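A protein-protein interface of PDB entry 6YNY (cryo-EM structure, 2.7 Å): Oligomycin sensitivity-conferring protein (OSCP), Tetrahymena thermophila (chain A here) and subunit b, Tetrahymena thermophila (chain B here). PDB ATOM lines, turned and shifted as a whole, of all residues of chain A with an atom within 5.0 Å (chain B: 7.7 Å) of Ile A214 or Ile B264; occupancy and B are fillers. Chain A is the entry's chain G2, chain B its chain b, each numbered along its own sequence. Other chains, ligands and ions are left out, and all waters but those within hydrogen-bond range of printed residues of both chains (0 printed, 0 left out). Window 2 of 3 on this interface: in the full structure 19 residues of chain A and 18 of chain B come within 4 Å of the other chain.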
ATOM      1  N   LEU A 210     -31.505 -15.696  27.657  1.00  0.00           N
ATOM      2  CA  LEU A 210     -30.892 -14.378  27.527  1.00  0.00           C
ATOM      3  C   LEU A 210     -29.414 -14.484  27.171  1.00  0.00           C
ATOM      4  O   LEU A 210     -28.932 -13.763  26.290  1.00  0.00           O
ATOM      5  CB  LEU A 210     -31.080 -13.583  28.819  1.00  0.00           C
ATOM      6  CG  LEU A 210     -32.395 -12.804  28.922  1.00  0.00           C
ATOM      7  CD1 LEU A 210     -33.601 -13.715  28.746  1.00  0.00           C
ATOM      8  CD2 LEU A 210     -32.471 -12.066  30.247  1.00  0.00           C
ATOM      9  N   LYS A 211     -28.678 -15.375  27.839  1.00  0.00           N
ATOM     10  CA  LYS A 211     -27.255 -15.515  27.545  1.00  0.00           C
ATOM     11  C   LYS A 211     -27.019 -15.906  26.093  1.00  0.00           C
ATOM     12  O   LYS A 211     -25.979 -15.562  25.519  1.00  0.00           O
ATOM     13  CB  LYS A 211     -26.623 -16.549  28.477  1.00  0.00           C
ATOM     14  CG  LYS A 211     -26.623 -16.147  29.943  1.00  0.00           C
ATOM     15  CD  LYS A 211     -25.716 -17.043  30.774  1.00  0.00           C
ATOM     16  CE  LYS A 211     -26.145 -18.501  30.708  1.00  0.00           C
ATOM     17  NZ  LYS A 211     -25.341 -19.359  31.619  1.00  0.00           N
ATOM     18  N   THR A 212     -27.965 -16.620  25.481  1.00  0.00           N
ATOM     19  CA  THR A 212     -27.812 -17.014  24.085  1.00  0.00           C
ATOM     20  C   THR A 212     -28.153 -15.866  23.142  1.00  0.00           C
ATOM     21  O   THR A 212     -27.442 -15.637  22.158  1.00  0.00           O
ATOM     22  CB  THR A 212     -28.691 -18.226  23.779  1.00  0.00           C
ATOM     23  OG1 THR A 212     -30.048 -17.946  24.146  1.00  0.00           O
ATOM     24  CG2 THR A 212     -28.199 -19.450  24.540  1.00  0.00           C
ATOM     25  N   GLU A 213     -29.233 -15.135  23.427  1.00  0.00           N
ATOM     26  CA  GLU A 213     -29.614 -14.020  22.566  1.00  0.00           C
ATOM     27  C   GLU A 213     -28.604 -12.883  22.655  1.00  0.00           C
ATOM     28  O   GLU A 213     -28.308 -12.228  21.650  1.00  0.00           O
ATOM     29  CB  GLU A 213     -31.012 -13.525  22.938  1.00  0.00           C
ATOM     30  CG  GLU A 213     -32.110 -14.556  22.735  1.00  0.00           C
ATOM     31  CD  GLU A 213     -32.351 -14.874  21.273  1.00  0.00           C
ATOM     32  OE1 GLU A 213     -31.806 -14.156  20.408  1.00  0.00           O
ATOM     33  OE2 GLU A 213     -33.086 -15.842  20.988  1.00  0.00           O
ATOM     34  N   ILE A 214     -28.064 -12.634  23.851  1.00  0.00           N
ATOM     35  CA  ILE A 214     -27.067 -11.579  24.008  1.00  0.00           C
ATOM     36  C   ILE A 214     -25.803 -11.915  23.230  1.00  0.00           C
ATOM     37  O   ILE A 214     -25.055 -11.016  22.827  1.00  0.00           O
ATOM     38  CB  ILE A 214     -26.767 -11.349  25.503  1.00  0.00           C
ATOM     39  CG1 ILE A 214     -28.012 -10.813  26.214  1.00  0.00           C
ATOM     40  CG2 ILE A 214     -25.597 -10.387  25.667  1.00  0.00           C
ATOM     41  CD1 ILE A 214     -27.896 -10.785  27.726  1.00  0.00           C
ATOM     42  N   ALA A 215     -25.538 -13.204  23.011  1.00  0.00           N
ATOM     43  CA  ALA A 215     -24.352 -13.597  22.258  1.00  0.00           C
ATOM     44  C   ALA A 215     -24.553 -13.412  20.759  1.00  0.00           C
ATOM     45  O   ALA A 215     -23.617 -13.032  20.047  1.00  0.00           O
ATOM     46  CB  ALA A 215     -23.992 -15.050  22.570  1.00  0.00           C
ATOM     47  N   LYS A 216     -25.762 -13.671  20.263  1.00  0.00           N
ATOM     48  CA  LYS A 216     -26.069 -13.573  18.843  1.00  0.00           C
ATOM     49  C   LYS A 216     -26.477 -12.165  18.426  1.00  0.00           C
ATOM     50  O   LYS A 216     -27.127 -12.000  17.386  1.00  0.00           O
ATOM     51  CB  LYS A 216     -27.172 -14.567  18.475  1.00  0.00           C
ATOM     52  CG  LYS A 216     -26.840 -16.010  18.820  1.00  0.00           C
ATOM     53  CD  LYS A 216     -27.865 -16.980  18.251  1.00  0.00           C
ATOM     54  CE  LYS A 216     -29.246 -16.760  18.851  1.00  0.00           C
ATOM     55  NZ  LYS A 216     -30.228 -17.768  18.364  1.00  0.00           N
ATOM     56  N   ILE A 217     -26.118 -11.148  19.213  1.00  0.00           N
ATOM     57  CA  ILE A 217     -26.461  -9.774  18.853  1.00  0.00           C
ATOM     58  C   ILE A 217     -25.900  -9.427  17.481  1.00  0.00           C
ATOM     59  O   ILE A 217     -26.520  -8.682  16.711  1.00  0.00           O
ATOM     60  CB  ILE A 217     -25.953  -8.799  19.934  1.00  0.00           C
ATOM     61  CG1 ILE A 217     -26.739  -8.979  21.237  1.00  0.00           C
ATOM     62  CG2 ILE A 217     -26.038  -7.362  19.438  1.00  0.00           C
ATOM     63  CD1 ILE A 217     -28.194  -8.548  21.161  1.00  0.00           C
ATOM     64  N   PHE A 219     -23.483  -7.522  16.721  1.00  0.00           N
ATOM     65  CA  PHE A 219     -23.215  -6.089  16.659  1.00  0.00           C
ATOM     66  C   PHE A 219     -22.122  -5.783  15.641  1.00  0.00           C
ATOM     67  O   PHE A 219     -22.089  -4.701  15.056  1.00  0.00           O
ATOM     68  CB  PHE A 219     -22.816  -5.556  18.037  1.00  0.00           C
ATOM     69  CG  PHE A 219     -21.680  -6.307  18.673  1.00  0.00           C
ATOM     70  CD1 PHE A 219     -20.367  -6.022  18.337  1.00  0.00           C
ATOM     71  CD2 PHE A 219     -21.925  -7.294  19.613  1.00  0.00           C
ATOM     72  CE1 PHE A 219     -19.321  -6.711  18.921  1.00  0.00           C
ATOM     73  CE2 PHE A 219     -20.884  -7.986  20.200  1.00  0.00           C
ATOM     74  CZ  PHE A 219     -19.581  -7.694  19.854  1.00  0.00           C
ATOM     75  N   ALA B 257     -15.479  -3.662  17.910  1.00  0.00           N
ATOM     76  CA  ALA B 257     -16.042  -4.948  18.307  1.00  0.00           C
ATOM     77  C   ALA B 257     -15.565  -5.354  19.695  1.00  0.00           C
ATOM     78  O   ALA B 257     -16.345  -5.879  20.499  1.00  0.00           O
ATOM     79  CB  ALA B 257     -15.676  -6.019  17.280  1.00  0.00           C
ATOM     80  N   ALA B 258     -14.286  -5.121  19.997  1.00  0.00           N
ATOM     81  CA  ALA B 258     -13.767  -5.465  21.315  1.00  0.00           C
ATOM     82  C   ALA B 258     -14.458  -4.658  22.406  1.00  0.00           C
ATOM     83  O   ALA B 258     -14.772  -5.188  23.478  1.00  0.00           O
ATOM     84  CB  ALA B 258     -12.256  -5.239  21.359  1.00  0.00           C
ATOM     85  N   LEU B 259     -14.705  -3.372  22.150  1.00  0.00           N
ATOM     86  CA  LEU B 259     -15.389  -2.537  23.133  1.00  0.00           C
ATOM     87  C   LEU B 259     -16.801  -3.047  23.394  1.00  0.00           C
ATOM     88  O   LEU B 259     -17.222  -3.184  24.548  1.00  0.00           O
ATOM     89  CB  LEU B 259     -15.417  -1.086  22.652  1.00  0.00           C
ATOM     90  CG  LEU B 259     -16.140  -0.086  23.556  1.00  0.00           C
ATOM     91  CD1 LEU B 259     -15.501  -0.045  24.936  1.00  0.00           C
ATOM     92  CD2 LEU B 259     -16.144   1.296  22.923  1.00  0.00           C
ATOM     93  N   LEU B 260     -17.549  -3.335  22.327  1.00  0.00           N
ATOM     94  CA  LEU B 260     -18.904  -3.849  22.498  1.00  0.00           C
ATOM     95  C   LEU B 260     -18.892  -5.237  23.125  1.00  0.00           C
ATOM     96  O   LEU B 260     -19.771  -5.569  23.929  1.00  0.00           O
ATOM     97  CB  LEU B 260     -19.628  -3.874  21.152  1.00  0.00           C
ATOM     98  CG  LEU B 260     -19.794  -2.523  20.453  1.00  0.00           C
ATOM     99  CD1 LEU B 260     -20.478  -2.701  19.108  1.00  0.00           C
ATOM    100  CD2 LEU B 260     -20.573  -1.547  21.324  1.00  0.00           C
ATOM    101  N   GLN B 261     -17.906  -6.064  22.769  1.00  0.00           N
ATOM    102  CA  GLN B 261     -17.807  -7.391  23.367  1.00  0.00           C
ATOM    103  C   GLN B 261     -17.670  -7.300  24.881  1.00  0.00           C
ATOM    104  O   GLN B 261     -18.220  -8.130  25.614  1.00  0.00           O
ATOM    105  CB  GLN B 261     -16.624  -8.149  22.764  1.00  0.00           C
ATOM    106  CG  GLN B 261     -16.416  -9.545  23.335  1.00  0.00           C
ATOM    107  CD  GLN B 261     -17.615 -10.449  23.125  1.00  0.00           C
ATOM    108  OE1 GLN B 261     -18.500 -10.151  22.323  1.00  0.00           O
ATOM    109  NE2 GLN B 261     -17.651 -11.562  23.849  1.00  0.00           N
ATOM    110  N   LYS B 262     -16.939  -6.294  25.368  1.00  0.00           N
ATOM    111  CA  LYS B 262     -16.816  -6.102  26.809  1.00  0.00           C
ATOM    112  C   LYS B 262     -18.173  -5.816  27.440  1.00  0.00           C
ATOM    113  O   LYS B 262     -18.462  -6.283  28.549  1.00  0.00           O
ATOM    114  CB  LYS B 262     -15.833  -4.970  27.102  1.00  0.00           C
ATOM    115  CG  LYS B 262     -15.647  -4.677  28.585  1.00  0.00           C
ATOM    116  CD  LYS B 262     -14.578  -3.620  28.820  1.00  0.00           C
ATOM    117  CE  LYS B 262     -13.181  -4.156  28.537  1.00  0.00           C
ATOM    118  NZ  LYS B 262     -12.126  -3.149  28.833  1.00  0.00           N
ATOM    119  N   LEU B 263     -19.018  -5.047  26.752  1.00  0.00           N
ATOM    120  CA  LEU B 263     -20.354  -4.767  27.268  1.00  0.00           C
ATOM    121  C   LEU B 263     -21.152  -6.054  27.432  1.00  0.00           C
ATOM    122  O   LEU B 263     -21.804  -6.269  28.460  1.00  0.00           O
ATOM    123  CB  LEU B 263     -21.079  -3.795  26.336  1.00  0.00           C
ATOM    124  CG  LEU B 263     -22.506  -3.409  26.736  1.00  0.00           C
ATOM    125  CD1 LEU B 263     -22.526  -2.744  28.104  1.00  0.00           C
ATOM    126  CD2 LEU B 263     -23.123  -2.499  25.686  1.00  0.00           C
ATOM    127  N   ILE B 264     -21.112  -6.925  26.421  1.00  0.00           N
ATOM    128  CA  ILE B 264     -21.792  -8.212  26.527  1.00  0.00           C
ATOM    129  C   ILE B 264     -21.171  -9.045  27.640  1.00  0.00           C
ATOM    130  O   ILE B 264     -21.874  -9.742  28.382  1.00  0.00           O
ATOM    131  CB  ILE B 264     -21.756  -8.950  25.175  1.00  0.00           C
ATOM    132  CG1 ILE B 264     -22.857  -8.428  24.247  1.00  0.00           C
ATOM    133  CG2 ILE B 264     -21.907 -10.454  25.374  1.00  0.00           C
ATOM    134  CD1 ILE B 264     -22.702  -6.976  23.852  1.00  0.00           C
ATOM    135  N   ASP B 265     -19.844  -8.987  27.776  1.00  0.00           N
ATOM    136  CA  ASP B 265     -19.181  -9.726  28.844  1.00  0.00           C
ATOM    137  C   ASP B 265     -19.601  -9.218  30.216  1.00  0.00           C
ATOM    138  O   ASP B 265     -19.711 -10.005  31.164  1.00  0.00           O
ATOM    139  CB  ASP B 265     -17.664  -9.627  28.686  1.00  0.00           C
ATOM    140  CG  ASP B 265     -16.915 -10.377  29.769  1.00  0.00           C
ATOM    141  OD1 ASP B 265     -16.958 -11.625  29.769  1.00  0.00           O
ATOM    142  OD2 ASP B 265     -16.284  -9.718  30.623  1.00  0.00           O
ATOM    143  N   ASP B 266     -19.841  -7.911  30.346  1.00  0.00           N
ATOM    144  CA  ASP B 266     -20.293  -7.369  31.623  1.00  0.00           C
ATOM    145  C   ASP B 266     -21.702  -7.845  31.954  1.00  0.00           C
ATOM    146  O   ASP B 266     -22.010  -8.131  33.116  1.00  0.00           O
ATOM    147  CB  ASP B 266     -20.237  -5.842  31.592  1.00  0.00           C
ATOM    148  CG  ASP B 266     -20.708  -5.214  32.889  1.00  0.00           C
ATOM    149  OD1 ASP B 266     -19.993  -5.341  33.904  1.00  0.00           O
ATOM    150  OD2 ASP B 266     -21.793  -4.597  32.893  1.00  0.00           O
ATOM    151  N   ALA B 267     -22.572  -7.935  30.945  1.00  0.00           N
ATOM    152  CA  ALA B 267     -23.931  -8.407  31.183  1.00  0.00           C
ATOM    153  C   ALA B 267     -23.934  -9.849  31.675  1.00  0.00           C
ATOM    154  O   ALA B 267     -24.661 -10.192  32.614  1.00  0.00           O
ATOM    155  CB  ALA B 267     -24.763  -8.275  29.908  1.00  0.00           C
ATOM    156  N   THR B 268     -23.126 -10.709  31.051  1.00  0.00           N
ATOM    157  CA  THR B 268     -23.074 -12.108  31.464  1.00  0.00           C
ATOM    158  C   THR B 268     -22.574 -12.242  32.897  1.00  0.00           C
ATOM    159  O   THR B 268     -23.098 -13.050  33.673  1.00  0.00           O
ATOM    160  CB  THR B 268     -22.180 -12.905  30.513  1.00  0.00           C
ATOM    161  OG1 THR B 268     -20.871 -12.322  30.479  1.00  0.00           O
ATOM    162  CG2 THR B 268     -22.767 -12.914  29.108  1.00  0.00           C
ATOM    163  N   SER B 269     -21.558 -11.459  33.268  1.00  0.00           N
ATOM    164  CA  SER B 269     -21.045 -11.518  34.632  1.00  0.00           C
ATOM    165  C   SER B 269     -22.097 -11.067  35.638  1.00  0.00           C
ATOM    166  O   SER B 269     -22.186 -11.617  36.742  1.00  0.00           O
ATOM    167  CB  SER B 269     -19.785 -10.660  34.755  1.00  0.00           C
ATOM    168  OG  SER B 269     -20.060  -9.304  34.448  1.00  0.00           O
ATOM    169  N   ALA B 270     -22.904 -10.068  35.275  1.00  0.00           N
ATOM    170  CA  ALA B 270     -23.964  -9.619  36.173  1.00  0.00           C
ATOM    171  C   ALA B 270     -24.951 -10.741  36.461  1.00  0.00           C
ATOM    172  O   ALA B 270     -25.438 -10.876  37.590  1.00  0.00           O
ATOM    173  CB  ALA B 270     -24.684  -8.413  35.570  1.00  0.00           C
ATOM    174  N   ILE B 271     -25.260 -11.559  35.453  1.00  0.00           N
ATOM    175  CA  ILE B 271     -26.164 -12.687  35.660  1.00  0.00           C
ATOM    176  C   ILE B 271     -25.557 -13.669  36.655  1.00  0.00           C
ATOM    177  O   ILE B 271     -26.222 -14.121  37.596  1.00  0.00           O
ATOM    178  CB  ILE B 271     -26.486 -13.371  34.319  1.00  0.00           C
ATOM    179  CG1 ILE B 271     -27.165 -12.380  33.370  1.00  0.00           C
ATOM    180  CG2 ILE B 271     -27.372 -14.591  34.544  1.00  0.00           C
ATOM    181  CD1 ILE B 271     -27.368 -12.912  31.966  1.00  0.00           C
ATOM    182  N   LEU B 308     -34.119  -9.541  33.480  1.00  0.00           N
ATOM    183  CA  LEU B 308     -34.045  -8.590  32.373  1.00  0.00           C
ATOM    184  C   LEU B 308     -33.784  -7.170  32.856  1.00  0.00           C
ATOM    185  O   LEU B 308     -32.809  -6.549  32.400  1.00  0.00           O
ATOM    186  CB  LEU B 308     -35.327  -8.680  31.540  1.00  0.00           C
ATOM    187  CG  LEU B 308     -35.423  -7.722  30.351  1.00  0.00           C
ATOM    188  CD1 LEU B 308     -34.273  -7.943  29.379  1.00  0.00           C
ATOM    189  CD2 LEU B 308     -36.761  -7.883  29.645  1.00  0.00           C
ATOM    190  N   ILE B 311     -30.141  -6.754  34.061  1.00  0.00           N
ATOM    191  CA  ILE B 311     -29.129  -6.676  33.013  1.00  0.00           C
ATOM    192  C   ILE B 311     -29.183  -5.322  32.317  1.00  0.00           C
ATOM    193  O   ILE B 311     -28.144  -4.716  32.028  1.00  0.00           O
ATOM    194  CB  ILE B 311     -29.313  -7.833  32.014  1.00  0.00           C
ATOM    195  CG1 ILE B 311     -29.130  -9.178  32.721  1.00  0.00           C
ATOM    196  CG2 ILE B 311     -28.330  -7.696  30.858  1.00  0.00           C
ATOM    197  CD1 ILE B 311     -29.638 -10.356  31.924  1.00  0.00           C
ATOM    198  N   ILE B 315     -26.281  -2.392  31.577  1.00  0.00           N
ATOM    199  CA  ILE B 315     -25.976  -1.962  30.216  1.00  0.00           C
ATOM    200  C   ILE B 315     -26.218  -0.465  30.066  1.00  0.00           C
ATOM    201  O   ILE B 315     -25.392   0.260  29.501  1.00  0.00           O
ATOM    202  CB  ILE B 315     -26.806  -2.772  29.202  1.00  0.00           C
ATOM    203  CG1 ILE B 315     -26.434  -4.256  29.282  1.00  0.00           C
ATOM    204  CG2 ILE B 315     -26.593  -2.232  27.791  1.00  0.00           C
ATOM    205  CD1 ILE B 315     -27.320  -5.162  28.452  1.00  0.00           C
ATOM    206  N   ASN B 318     -23.312   1.661  31.269  1.00  0.00           N
ATOM    207  CA  ASN B 318     -22.199   1.790  30.335  1.00  0.00           C
ATOM    208  C   ASN B 318     -22.554   2.716  29.179  1.00  0.00           C
ATOM    209  O   ASN B 318     -21.713   3.499  28.723  1.00  0.00           O
ATOM    210  CB  ASN B 318     -21.795   0.412  29.812  1.00  0.00           C
ATOM    211  CG  ASN B 318     -21.366  -0.528  30.921  1.00  0.00           C
ATOM    212  OD1 ASN B 318     -21.700  -0.324  32.088  1.00  0.00           O
ATOM    213  ND2 ASN B 318     -20.625  -1.569  30.561  1.00  0.00           N
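Of the 19 printed residues of chain B, 6 touch a printed residue of chain A.
Hydrophobic or aromatic side chains of chain B that line the printed part of chain A: Leu B260, Ile B264, Ile B271 and Ile B311.
Of the 9 printed residues of chain A, 4 touch a printed residue of chain B.
Printed residues of chain A that touch a printed residue of chain B: Leu A210, Lys A211, Ile A214 and Phe A219.
Among the printed residues, 6 pairs touch across the chains.
Among the printed residues, no Asp or Glu carboxylate lies within 4 Å of a Lys or Arg side-chain nitrogen of the other chain.
Among the printed residues, merely in contact across the chains: Phe A219 with Leu B260 (3.4 Å), Phe A219 with Ala B257 (3.5 Å), Phe A219 with Gln B261 (3.6 Å), Ile A214 with Ile B264 (3.7 Å), Leu A210 with Ile B311 (3.7 Å) and Lys A211 with Ile B271 (3.9 Å).
Of the printed residues of chain B, Leu A210 touches Ile B311.
Of the printed residues of chain B, Lys A211 touches Ile B271.
Ile A214 touches one residue of chain B.
Ala A215 touches none of the printed residues of chain B.
Ile A217 touches none of the printed residues of chain B.
Of the printed residues of chain B, Phe A219 touches Ala B257, Leu B260 and Gln B261.
Printed residues of chain A within 4 Å of Ile B264: Ile A214.
Of the printed residues of chain A, Ile B271 touches Lys A211 (3.9 Å).
The nearest residue of chain A that does not touch Ile B264 is Phe A219 (4.2 Å).
The nearest printed residue of chain B that does not touch Phe A219 is Ile B264 (4.2 Å).
O of Ile B264 lies close to OG1 of Thr B268 (3.5 Å).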
